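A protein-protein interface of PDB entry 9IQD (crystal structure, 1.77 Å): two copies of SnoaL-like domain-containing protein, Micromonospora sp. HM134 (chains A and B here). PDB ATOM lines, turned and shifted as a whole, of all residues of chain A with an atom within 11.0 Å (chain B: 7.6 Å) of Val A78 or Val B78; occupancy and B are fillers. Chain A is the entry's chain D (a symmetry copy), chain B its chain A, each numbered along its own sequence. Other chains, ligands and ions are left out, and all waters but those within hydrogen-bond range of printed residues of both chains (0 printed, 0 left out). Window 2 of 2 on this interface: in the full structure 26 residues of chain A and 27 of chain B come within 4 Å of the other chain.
The backbone carbonyl oxygen of Ile B76 is in hydrogen-bond range of the backbone NH of Phe B83 (2.7 Å).
The backbone carbonyl oxygen (O) of Ile A76 lies within hydrogen-bond range of the backbone NH (N) of Phe A83, 2.9 Å away.
Among the printed residues, pairs that only touch across the chains: Ile A76 with Val B78, Ile A76 with Arg B81, Ile A76 with Phe B83, Val A78 with Ile B76, Val A78 with Val B78 and Phe A83 with Phe B83.
Of the printed residues of chain A, Val B78 touches Ile A76 (3.8 Å) and Val A78 (2.8 Å).
No residue of chain B comes within 4 Å of Ala A79.
Of the printed residues of chain A, Ile B76 touches Val A78 (3.6 Å).
No residue of chain A comes within 4 Å of Val B77.
No residue of chain A comes within 4 Å of Ala B79.
No residue of chain A comes within 4 Å of Asp B80.
Printed residues of chain B within 4 Å of Phe A83: Phe B83 (3.6 Å).
Of the printed residues of chain A, Phe B83 touches Ile A76 and Phe A83.
Of the printed residues of chain A, Arg B81 touches Ile A76.
Val A102 touches none of the printed residues of chain B.
Val A77 touches none of the printed residues of chain B.
The nearest residue of chain B that does not touch Val A78 is Val B77 (4.8 Å).
The nearest printed residue of chain B that does not touch Ile A76 is Ile B76 (6.7 Å).
Hydrophobic or aromatic side chains of chain B within 4 Å of the printed part of chain A: Ile B76, Val B78 and Phe B83.
Printed residues of chain A that touch a printed residue of chain B: Ile A76, Val A78 and Phe A83.
Ile A76 touches Val B78, and with the chains exchanged Val A78 touches Ile B76.
Ile A76 touches Arg B81, but with the chains exchanged Arg A81 does not touch Ile B76 (4.6 Å).
Ile A76 touches Phe B83, but with the chains exchanged Phe A83 does not touch Ile B76 (4.05 Å).
Val A78 touches its own counterpart, Val B78.
Positions printed for both chains: 75, 76, 77, 78, 79, 80, 81, 82, 83 and 103.
Of the 6 pairs that touch across the chains among the printed residues, 4 have their exchanged pair printed and touching as well.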
ATOM      1  N   SER A   5      -3.040   5.378  22.547  1.00  0.00           N
ATOM      2  CA  SER A   5      -2.911   4.547  21.352  1.00  0.00           C
ATOM      3  C   SER A   5      -3.552   5.230  20.140  1.00  0.00           C
ATOM      4  O   SER A   5      -4.653   5.791  20.248  1.00  0.00           O
ATOM      5  CB  SER A   5      -3.566   3.182  21.586  1.00  0.00           C
ATOM      6  OG  SER A   5      -4.100   2.664  20.370  1.00  0.00           O
ATOM      7  N   VAL A   7      -4.947   3.844  17.729  1.00  0.00           N
ATOM      8  CA  VAL A   7      -6.213   3.169  17.454  1.00  0.00           C
ATOM      9  C   VAL A   7      -7.329   3.804  18.274  1.00  0.00           C
ATOM     10  O   VAL A   7      -8.380   4.177  17.742  1.00  0.00           O
ATOM     11  CB  VAL A   7      -6.082   1.662  17.737  1.00  0.00           C
ATOM     12  CG1 VAL A   7      -7.416   0.954  17.504  1.00  0.00           C
ATOM     13  CG2 VAL A   7      -4.968   1.053  16.883  1.00  0.00           C
ATOM     14  N   ASP A  74     -13.103  -5.579  22.652  1.00  0.00           N
ATOM     15  CA  ASP A  74     -12.049  -4.832  23.303  1.00  0.00           C
ATOM     16  C   ASP A  74     -10.826  -4.825  22.402  1.00  0.00           C
ATOM     17  O   ASP A  74     -10.559  -5.795  21.686  1.00  0.00           O
ATOM     18  CB  ASP A  74     -11.692  -5.464  24.647  1.00  0.00           C
ATOM     19  CG  ASP A  74     -12.811  -5.344  25.650  1.00  0.00           C
ATOM     20  OD1 ASP A  74     -13.247  -6.402  26.156  1.00  0.00           O
ATOM     21  OD2 ASP A  74     -13.297  -4.218  25.885  1.00  0.00           O
ATOM     22  N   ARG A  75     -10.089  -3.712  22.433  1.00  0.00           N
ATOM     23  CA  ARG A  75      -8.803  -3.649  21.750  1.00  0.00           C
ATOM     24  C   ARG A  75      -7.830  -4.582  22.464  1.00  0.00           C
ATOM     25  O   ARG A  75      -7.606  -4.445  23.671  1.00  0.00           O
ATOM     26  CB  ARG A  75      -8.267  -2.212  21.746  1.00  0.00           C
ATOM     27  CG  ARG A  75      -9.135  -1.204  20.983  1.00  0.00           C
ATOM     28  CD  ARG A  75      -8.810   0.252  21.392  1.00  0.00           C
ATOM     29  NE  ARG A  75      -7.371   0.399  21.550  1.00  0.00           N
ATOM     30  CZ  ARG A  75      -6.755   0.814  22.647  1.00  0.00           C
ATOM     31  NH1 ARG A  75      -7.428   1.295  23.685  1.00  0.00           N
ATOM     32  NH2 ARG A  75      -5.428   0.751  22.701  1.00  0.00           N
ATOM     33  N   ILE A  76      -7.275  -5.543  21.736  1.00  0.00           N
ATOM     34  CA  ILE A  76      -6.301  -6.483  22.279  1.00  0.00           C
ATOM     35  C   ILE A  76      -4.932  -6.018  21.802  1.00  0.00           C
ATOM     36  O   ILE A  76      -4.649  -6.023  20.598  1.00  0.00           O
ATOM     37  CB  ILE A  76      -6.593  -7.931  21.845  1.00  0.00           C
ATOM     38  CG1 ILE A  76      -8.014  -8.336  22.247  1.00  0.00           C
ATOM     39  CG2 ILE A  76      -5.590  -8.897  22.483  1.00  0.00           C
ATOM     40  CD1 ILE A  76      -8.253  -8.348  23.742  1.00  0.00           C
ATOM     41  N   VAL A  77      -4.079  -5.608  22.743  1.00  0.00           N
ATOM     42  CA  VAL A  77      -2.819  -4.924  22.455  1.00  0.00           C
ATOM     43  C   VAL A  77      -1.664  -5.867  22.754  1.00  0.00           C
ATOM     44  O   VAL A  77      -1.613  -6.455  23.840  1.00  0.00           O
ATOM     45  CB  VAL A  77      -2.692  -3.631  23.283  1.00  0.00           C
ATOM     46  CG1 VAL A  77      -1.466  -2.846  22.862  1.00  0.00           C
ATOM     47  CG2 VAL A  77      -3.947  -2.765  23.126  1.00  0.00           C
ATOM     48  N   VAL A  78      -0.743  -6.021  21.793  1.00  0.00           N
ATOM     49  CA  VAL A  78       0.425  -6.900  21.929  1.00  0.00           C
ATOM     50  C   VAL A  78       1.465  -6.658  20.849  1.00  0.00           C
ATOM     51  O   VAL A  78       1.143  -6.601  19.656  1.00  0.00           O
ATOM     52  CB  VAL A  78       0.043  -8.389  21.905  1.00  0.00           C
ATOM     53  CG1 VAL A  78      -0.538  -8.790  23.214  1.00  0.00           C
ATOM     54  CG2 VAL A  78      -0.941  -8.661  20.769  1.00  0.00           C
ATOM     55  N   ALA A  79       2.729  -6.590  21.259  1.00  0.00           N
ATOM     56  CA  ALA A  79       3.836  -6.340  20.338  1.00  0.00           C
ATOM     57  C   ALA A  79       3.578  -4.966  19.718  1.00  0.00           C
ATOM     58  O   ALA A  79       3.279  -4.014  20.452  1.00  0.00           O
ATOM     59  CB  ALA A  79       3.955  -7.505  19.359  1.00  0.00           C
ATOM     60  N   ASP A  80       3.674  -4.815  18.402  1.00  0.00           N
ATOM     61  CA  ASP A  80       3.413  -3.541  17.747  1.00  0.00           C
ATOM     62  C   ASP A  80       2.041  -3.537  17.093  1.00  0.00           C
ATOM     63  O   ASP A  80       1.872  -2.966  16.018  1.00  0.00           O
ATOM     64  CB  ASP A  80       4.507  -3.245  16.722  1.00  0.00           C
ATOM     65  CG  ASP A  80       4.556  -4.278  15.583  1.00  0.00           C
ATOM     66  OD1 ASP A  80       4.017  -5.403  15.729  1.00  0.00           O
ATOM     67  OD2 ASP A  80       5.157  -3.955  14.533  1.00  0.00           O
ATOM     68  N   ARG A  81       1.052  -4.180  17.717  1.00  0.00           N
ATOM     69  CA  ARG A  81      -0.189  -4.532  17.036  1.00  0.00           C
ATOM     70  C   ARG A  81      -1.384  -4.428  17.972  1.00  0.00           C
ATOM     71  O   ARG A  81      -1.266  -4.589  19.188  1.00  0.00           O
ATOM     72  CB  ARG A  81      -0.112  -5.954  16.482  1.00  0.00           C
ATOM     73  CG  ARG A  81       0.275  -5.989  15.027  1.00  0.00           C
ATOM     74  CD  ARG A  81       0.797  -7.336  14.607  1.00  0.00           C
ATOM     75  NE  ARG A  81       0.238  -7.716  13.317  1.00  0.00           N
ATOM     76  CZ  ARG A  81       0.947  -7.778  12.200  1.00  0.00           C
ATOM     77  NH1 ARG A  81       2.222  -7.416  12.170  1.00  0.00           N
ATOM     78  NH2 ARG A  81       0.359  -8.192  11.081  1.00  0.00           N
ATOM     79  N   GLU A  82      -2.552  -4.170  17.382  1.00  0.00           N
ATOM     80  CA  GLU A  82      -3.807  -4.244  18.107  1.00  0.00           C
ATOM     81  C   GLU A  82      -4.784  -5.028  17.251  1.00  0.00           C
ATOM     82  O   GLU A  82      -4.770  -4.903  16.027  1.00  0.00           O
ATOM     83  CB  GLU A  82      -4.395  -2.856  18.432  1.00  0.00           C
ATOM     84  CG  GLU A  82      -3.435  -1.967  19.257  1.00  0.00           C
ATOM     85  CD  GLU A  82      -4.122  -0.759  19.882  1.00  0.00           C
ATOM     86  OE1 GLU A  82      -5.370  -0.762  19.984  1.00  0.00           O
ATOM     87  OE2 GLU A  82      -3.410   0.195  20.279  1.00  0.00           O
ATOM     88  N   PHE A  83      -5.607  -5.838  17.905  1.00  0.00           N
ATOM     89  CA  PHE A  83      -6.655  -6.616  17.256  1.00  0.00           C
ATOM     90  C   PHE A  83      -7.996  -6.139  17.779  1.00  0.00           C
ATOM     91  O   PHE A  83      -8.167  -5.978  18.994  1.00  0.00           O
ATOM     92  CB  PHE A  83      -6.499  -8.112  17.544  1.00  0.00           C
ATOM     93  CG  PHE A  83      -5.181  -8.679  17.108  1.00  0.00           C
ATOM     94  CD1 PHE A  83      -4.088  -8.655  17.949  1.00  0.00           C
ATOM     95  CD2 PHE A  83      -5.039  -9.234  15.846  1.00  0.00           C
ATOM     96  CE1 PHE A  83      -2.875  -9.168  17.542  1.00  0.00           C
ATOM     97  CE2 PHE A  83      -3.839  -9.752  15.441  1.00  0.00           C
ATOM     98  CZ  PHE A  83      -2.753  -9.716  16.287  1.00  0.00           C
ATOM     99  N   LEU A  84      -8.954  -5.932  16.878  1.00  0.00           N
ATOM    100  CA  LEU A  84     -10.243  -5.370  17.269  1.00  0.00           C
ATOM    101  C   LEU A  84     -11.342  -6.031  16.450  1.00  0.00           C
ATOM    102  O   LEU A  84     -11.446  -5.773  15.247  1.00  0.00           O
ATOM    103  CB  LEU A  84     -10.257  -3.862  17.054  1.00  0.00           C
ATOM    104  CG  LEU A  84     -11.574  -3.170  17.393  1.00  0.00           C
ATOM    105  CD1 LEU A  84     -11.911  -3.408  18.865  1.00  0.00           C
ATOM    106  CD2 LEU A  84     -11.441  -1.703  17.090  1.00  0.00           C
ATOM    107  N   GLU A  85     -12.172  -6.844  17.097  1.00  0.00           N
ATOM    108  CA  GLU A  85     -13.344  -7.396  16.423  1.00  0.00           C
ATOM    109  C   GLU A  85     -14.478  -6.374  16.380  1.00  0.00           C
ATOM    110  O   GLU A  85     -14.603  -5.501  17.253  1.00  0.00           O
ATOM    111  CB  GLU A  85     -13.818  -8.672  17.115  1.00  0.00           C
ATOM    112  CG  GLU A  85     -12.886  -9.843  16.875  1.00  0.00           C
ATOM    113  CD  GLU A  85     -13.483 -11.175  17.317  1.00  0.00           C
ATOM    114  OE1 GLU A  85     -14.574 -11.569  16.842  1.00  0.00           O
ATOM    115  OE2 GLU A  85     -12.848 -11.829  18.164  1.00  0.00           O
ATOM    116  N   ASP A 101     -10.303  -6.046  12.736  1.00  0.00           N
ATOM    117  CA  ASP A 101      -9.255  -5.134  12.288  1.00  0.00           C
ATOM    118  C   ASP A 101      -7.936  -5.568  12.908  1.00  0.00           C
ATOM    119  O   ASP A 101      -7.873  -5.806  14.119  1.00  0.00           O
ATOM    120  CB  ASP A 101      -9.527  -3.683  12.712  1.00  0.00           C
ATOM    121  CG  ASP A 101     -10.731  -3.061  12.037  1.00  0.00           C
ATOM    122  OD1 ASP A 101     -11.088  -3.480  10.916  1.00  0.00           O
ATOM    123  OD2 ASP A 101     -11.304  -2.114  12.635  1.00  0.00           O
ATOM    124  N   VAL A 102      -6.885  -5.635  12.101  1.00  0.00           N
ATOM    125  CA  VAL A 102      -5.546  -5.906  12.602  1.00  0.00           C
ATOM    126  C   VAL A 102      -4.732  -4.649  12.349  1.00  0.00           C
ATOM    127  O   VAL A 102      -4.499  -4.281  11.195  1.00  0.00           O
ATOM    128  CB  VAL A 102      -4.916  -7.132  11.927  1.00  0.00           C
ATOM    129  CG1 VAL A 102      -3.482  -7.322  12.419  1.00  0.00           C
ATOM    130  CG2 VAL A 102      -5.769  -8.376  12.226  1.00  0.00           C
ATOM    131  N   PHE A 103      -4.306  -3.986  13.422  1.00  0.00           N
ATOM    132  CA  PHE A 103      -3.549  -2.745  13.339  1.00  0.00           C
ATOM    133  C   PHE A 103      -2.074  -3.024  13.588  1.00  0.00           C
ATOM    134  O   PHE A 103      -1.721  -3.626  14.608  1.00  0.00           O
ATOM    135  CB  PHE A 103      -4.033  -1.725  14.373  1.00  0.00           C
ATOM    136  CG  PHE A 103      -5.428  -1.229  14.158  1.00  0.00           C
ATOM    137  CD1 PHE A 103      -6.511  -1.868  14.746  1.00  0.00           C
ATOM    138  CD2 PHE A 103      -5.655  -0.086  13.403  1.00  0.00           C
ATOM    139  CE1 PHE A 103      -7.789  -1.386  14.564  1.00  0.00           C
ATOM    140  CE2 PHE A 103      -6.934   0.401  13.215  1.00  0.00           C
ATOM    141  CZ  PHE A 103      -8.005  -0.248  13.796  1.00  0.00           C
ATOM    142  N   THR A 104      -1.221  -2.587  12.664  1.00  0.00           N
ATOM    143  CA  THR A 104       0.220  -2.558  12.882  1.00  0.00           C
ATOM    144  C   THR A 104       0.617  -1.122  13.202  1.00  0.00           C
ATOM    145  O   THR A 104       0.240  -0.196  12.477  1.00  0.00           O
ATOM    146  CB  THR A 104       0.974  -3.065  11.653  1.00  0.00           C
ATOM    147  OG1 THR A 104       0.588  -4.418  11.399  1.00  0.00           O
ATOM    148  CG2 THR A 104       2.513  -2.988  11.871  1.00  0.00           C
ATOM    149  N   LEU A 105       1.321  -0.931  14.309  1.00  0.00           N
ATOM    150  CA  LEU A 105       1.647   0.407  14.779  1.00  0.00           C
ATOM    151  C   LEU A 105       3.143   0.659  14.640  1.00  0.00           C
ATOM    152  O   LEU A 105       3.950  -0.271  14.668  1.00  0.00           O
ATOM    153  CB  LEU A 105       1.244   0.604  16.239  1.00  0.00           C
ATOM    154  CG  LEU A 105      -0.233   0.336  16.563  1.00  0.00           C
ATOM    155  CD1 LEU A 105      -0.521   0.760  18.019  1.00  0.00           C
ATOM    156  CD2 LEU A 105      -1.154   1.011  15.566  1.00  0.00           C
ATOM    157  N   ARG A 106       3.499   1.934  14.498  1.00  0.00           N
ATOM    158  CA  ARG A 106       4.895   2.346  14.418  1.00  0.00           C
ATOM    159  C   ARG A 106       4.992   3.783  14.905  1.00  0.00           C
ATOM    160  O   ARG A 106       4.343   4.673  14.348  1.00  0.00           O
ATOM    161  CB  ARG A 106       5.426   2.224  12.990  1.00  0.00           C
ATOM    162  CG  ARG A 106       6.754   2.960  12.758  1.00  0.00           C
ATOM    163  CD  ARG A 106       7.608   2.216  11.751  1.00  0.00           C
ATOM    164  NE  ARG A 106       7.463   2.849  10.444  1.00  0.00           N
ATOM    165  CZ  ARG A 106       7.715   2.254   9.287  1.00  0.00           C
ATOM    166  NH1 ARG A 106       8.182   1.015   9.231  1.00  0.00           N
ATOM    167  NH2 ARG A 106       7.478   2.913   8.155  1.00  0.00           N
ATOM    168  N   ARG B  75       2.271 -16.763  15.588  1.00  0.00           N
ATOM    169  CA  ARG B  75       1.137 -17.065  16.451  1.00  0.00           C
ATOM    170  C   ARG B  75       1.238 -16.201  17.702  1.00  0.00           C
ATOM    171  O   ARG B  75       2.204 -16.318  18.468  1.00  0.00           O
ATOM    172  CB  ARG B  75       1.095 -18.549  16.812  1.00  0.00           C
ATOM    173  CG  ARG B  75      -0.122 -18.937  17.638  1.00  0.00           C
ATOM    174  CD  ARG B  75      -0.345 -20.459  17.621  1.00  0.00           C
ATOM    175  NE  ARG B  75       0.864 -21.169  18.025  1.00  0.00           N
ATOM    176  CZ  ARG B  75       1.268 -21.266  19.283  1.00  0.00           C
ATOM    177  NH1 ARG B  75       0.542 -20.780  20.278  1.00  0.00           N
ATOM    178  NH2 ARG B  75       2.436 -21.848  19.548  1.00  0.00           N
ATOM    179  N   ILE B  76       0.254 -15.328  17.903  1.00  0.00           N
ATOM    180  CA  ILE B  76       0.271 -14.337  18.980  1.00  0.00           C
ATOM    181  C   ILE B  76      -0.751 -14.756  20.032  1.00  0.00           C
ATOM    182  O   ILE B  76      -1.909 -15.055  19.702  1.00  0.00           O
ATOM    183  CB  ILE B  76      -0.024 -12.930  18.428  1.00  0.00           C
ATOM    184  CG1 ILE B  76       1.191 -12.396  17.673  1.00  0.00           C
ATOM    185  CG2 ILE B  76      -0.372 -11.946  19.538  1.00  0.00           C
ATOM    186  CD1 ILE B  76       0.834 -11.587  16.467  1.00  0.00           C
ATOM    187  N   VAL B  77      -0.331 -14.791  21.297  1.00  0.00           N
ATOM    188  CA  VAL B  77      -1.188 -15.235  22.396  1.00  0.00           C
ATOM    189  C   VAL B  77      -1.357 -14.098  23.397  1.00  0.00           C
ATOM    190  O   VAL B  77      -0.363 -13.536  23.865  1.00  0.00           O
ATOM    191  CB  VAL B  77      -0.607 -16.478  23.089  1.00  0.00           C
ATOM    192  CG1 VAL B  77      -1.486 -16.889  24.257  1.00  0.00           C
ATOM    193  CG2 VAL B  77      -0.472 -17.630  22.095  1.00  0.00           C
ATOM    194  N   VAL B  78      -2.612 -13.788  23.745  1.00  0.00           N
ATOM    195  CA  VAL B  78      -2.952 -12.820  24.789  1.00  0.00           C
ATOM    196  C   VAL B  78      -4.087 -13.405  25.614  1.00  0.00           C
ATOM    197  O   VAL B  78      -5.206 -13.571  25.104  1.00  0.00           O
ATOM    198  CB  VAL B  78      -3.367 -11.449  24.231  1.00  0.00           C
ATOM    199  CG1 VAL B  78      -3.565 -10.460  25.379  1.00  0.00           C
ATOM    200  CG2 VAL B  78      -2.363 -10.943  23.242  1.00  0.00           C
ATOM    201  N   ALA B  79      -3.815 -13.706  26.881  1.00  0.00           N
ATOM    202  CA  ALA B  79      -4.815 -14.314  27.752  1.00  0.00           C
ATOM    203  C   ALA B  79      -5.405 -15.545  27.076  1.00  0.00           C
ATOM    204  O   ALA B  79      -4.664 -16.457  26.687  1.00  0.00           O
ATOM    205  CB  ALA B  79      -5.915 -13.311  28.109  1.00  0.00           C
ATOM    206  N   ASP B  80      -6.731 -15.574  26.920  1.00  0.00           N
ATOM    207  CA  ASP B  80      -7.424 -16.719  26.330  1.00  0.00           C
ATOM    208  C   ASP B  80      -7.641 -16.606  24.822  1.00  0.00           C
ATOM    209  O   ASP B  80      -8.464 -17.352  24.277  1.00  0.00           O
ATOM    210  CB  ASP B  80      -8.781 -16.931  27.004  1.00  0.00           C
ATOM    211  CG  ASP B  80      -9.646 -15.679  26.979  1.00  0.00           C
ATOM    212  OD1 ASP B  80     -10.870 -15.804  27.206  1.00  0.00           O
ATOM    213  OD2 ASP B  80      -9.098 -14.556  26.803  1.00  0.00           O
ATOM    214  N   ARG B  81      -6.938 -15.714  24.134  1.00  0.00           N
ATOM    215  CA  ARG B  81      -7.060 -15.606  22.684  1.00  0.00           C
ATOM    216  C   ARG B  81      -5.718 -15.867  22.013  1.00  0.00           C
ATOM    217  O   ARG B  81      -4.664 -15.562  22.572  1.00  0.00           O
ATOM    218  CB  ARG B  81      -7.594 -14.225  22.278  1.00  0.00           C
ATOM    219  CG  ARG B  81      -8.917 -13.874  22.952  1.00  0.00           C
ATOM    220  CD  ARG B  81      -9.672 -12.792  22.180  1.00  0.00           C
ATOM    221  NE  ARG B  81     -10.931 -12.424  22.824  1.00  0.00           N
ATOM    222  CZ  ARG B  81     -11.038 -11.744  23.961  1.00  0.00           C
ATOM    223  NH1 ARG B  81      -9.973 -11.293  24.604  1.00  0.00           N
ATOM    224  NH2 ARG B  81     -12.247 -11.508  24.463  1.00  0.00           N
ATOM    225  N   GLU B  82      -5.762 -16.454  20.809  1.00  0.00           N
ATOM    226  CA  GLU B  82      -4.589 -16.579  19.949  1.00  0.00           C
ATOM    227  C   GLU B  82      -4.957 -16.013  18.586  1.00  0.00           C
ATOM    228  O   GLU B  82      -6.094 -16.177  18.132  1.00  0.00           O
ATOM    229  CB  GLU B  82      -4.102 -18.039  19.790  1.00  0.00           C
ATOM    230  CG  GLU B  82      -3.986 -18.852  21.104  1.00  0.00           C
ATOM    231  CD  GLU B  82      -2.873 -19.911  21.048  1.00  0.00           C
ATOM    232  OE1 GLU B  82      -2.695 -20.664  22.036  1.00  0.00           O
ATOM    233  OE2 GLU B  82      -2.192 -20.003  20.004  1.00  0.00           O
ATOM    234  N   PHE B  83      -4.007 -15.333  17.949  1.00  0.00           N
ATOM    235  CA  PHE B  83      -4.219 -14.720  16.642  1.00  0.00           C
ATOM    236  C   PHE B  83      -3.185 -15.243  15.660  1.00  0.00           C
ATOM    237  O   PHE B  83      -2.003 -15.333  15.992  1.00  0.00           O
ATOM    238  CB  PHE B  83      -4.127 -13.191  16.729  1.00  0.00           C
ATOM    239  CG  PHE B  83      -5.022 -12.596  17.777  1.00  0.00           C
ATOM    240  CD1 PHE B  83      -4.576 -12.447  19.086  1.00  0.00           C
ATOM    241  CD2 PHE B  83      -6.311 -12.210  17.464  1.00  0.00           C
ATOM    242  CE1 PHE B  83      -5.402 -11.920  20.051  1.00  0.00           C
ATOM    243  CE2 PHE B  83      -7.138 -11.671  18.430  1.00  0.00           C
ATOM    244  CZ  PHE B  83      -6.688 -11.528  19.716  1.00  0.00           C
ATOM    245  N   PHE B 103      -8.569 -17.382  17.663  1.00  0.00           N
ATOM    246  CA  PHE B 103      -8.937 -18.504  18.504  1.00  0.00           C
ATOM    247  C   PHE B 103      -9.370 -17.975  19.865  1.00  0.00           C
ATOM    248  O   PHE B 103      -8.792 -17.013  20.384  1.00  0.00           O
ATOM    249  CB  PHE B 103      -7.768 -19.476  18.684  1.00  0.00           C
ATOM    250  CG  PHE B 103      -7.293 -20.119  17.412  1.00  0.00           C
ATOM    251  CD1 PHE B 103      -6.367 -19.480  16.606  1.00  0.00           C
ATOM    252  CD2 PHE B 103      -7.764 -21.381  17.029  1.00  0.00           C
ATOM    253  CE1 PHE B 103      -5.896 -20.084  15.450  1.00  0.00           C
ATOM    254  CE2 PHE B 103      -7.303 -21.992  15.885  1.00  0.00           C
ATOM    255  CZ  PHE B 103      -6.385 -21.337  15.070  1.00  0.00           C
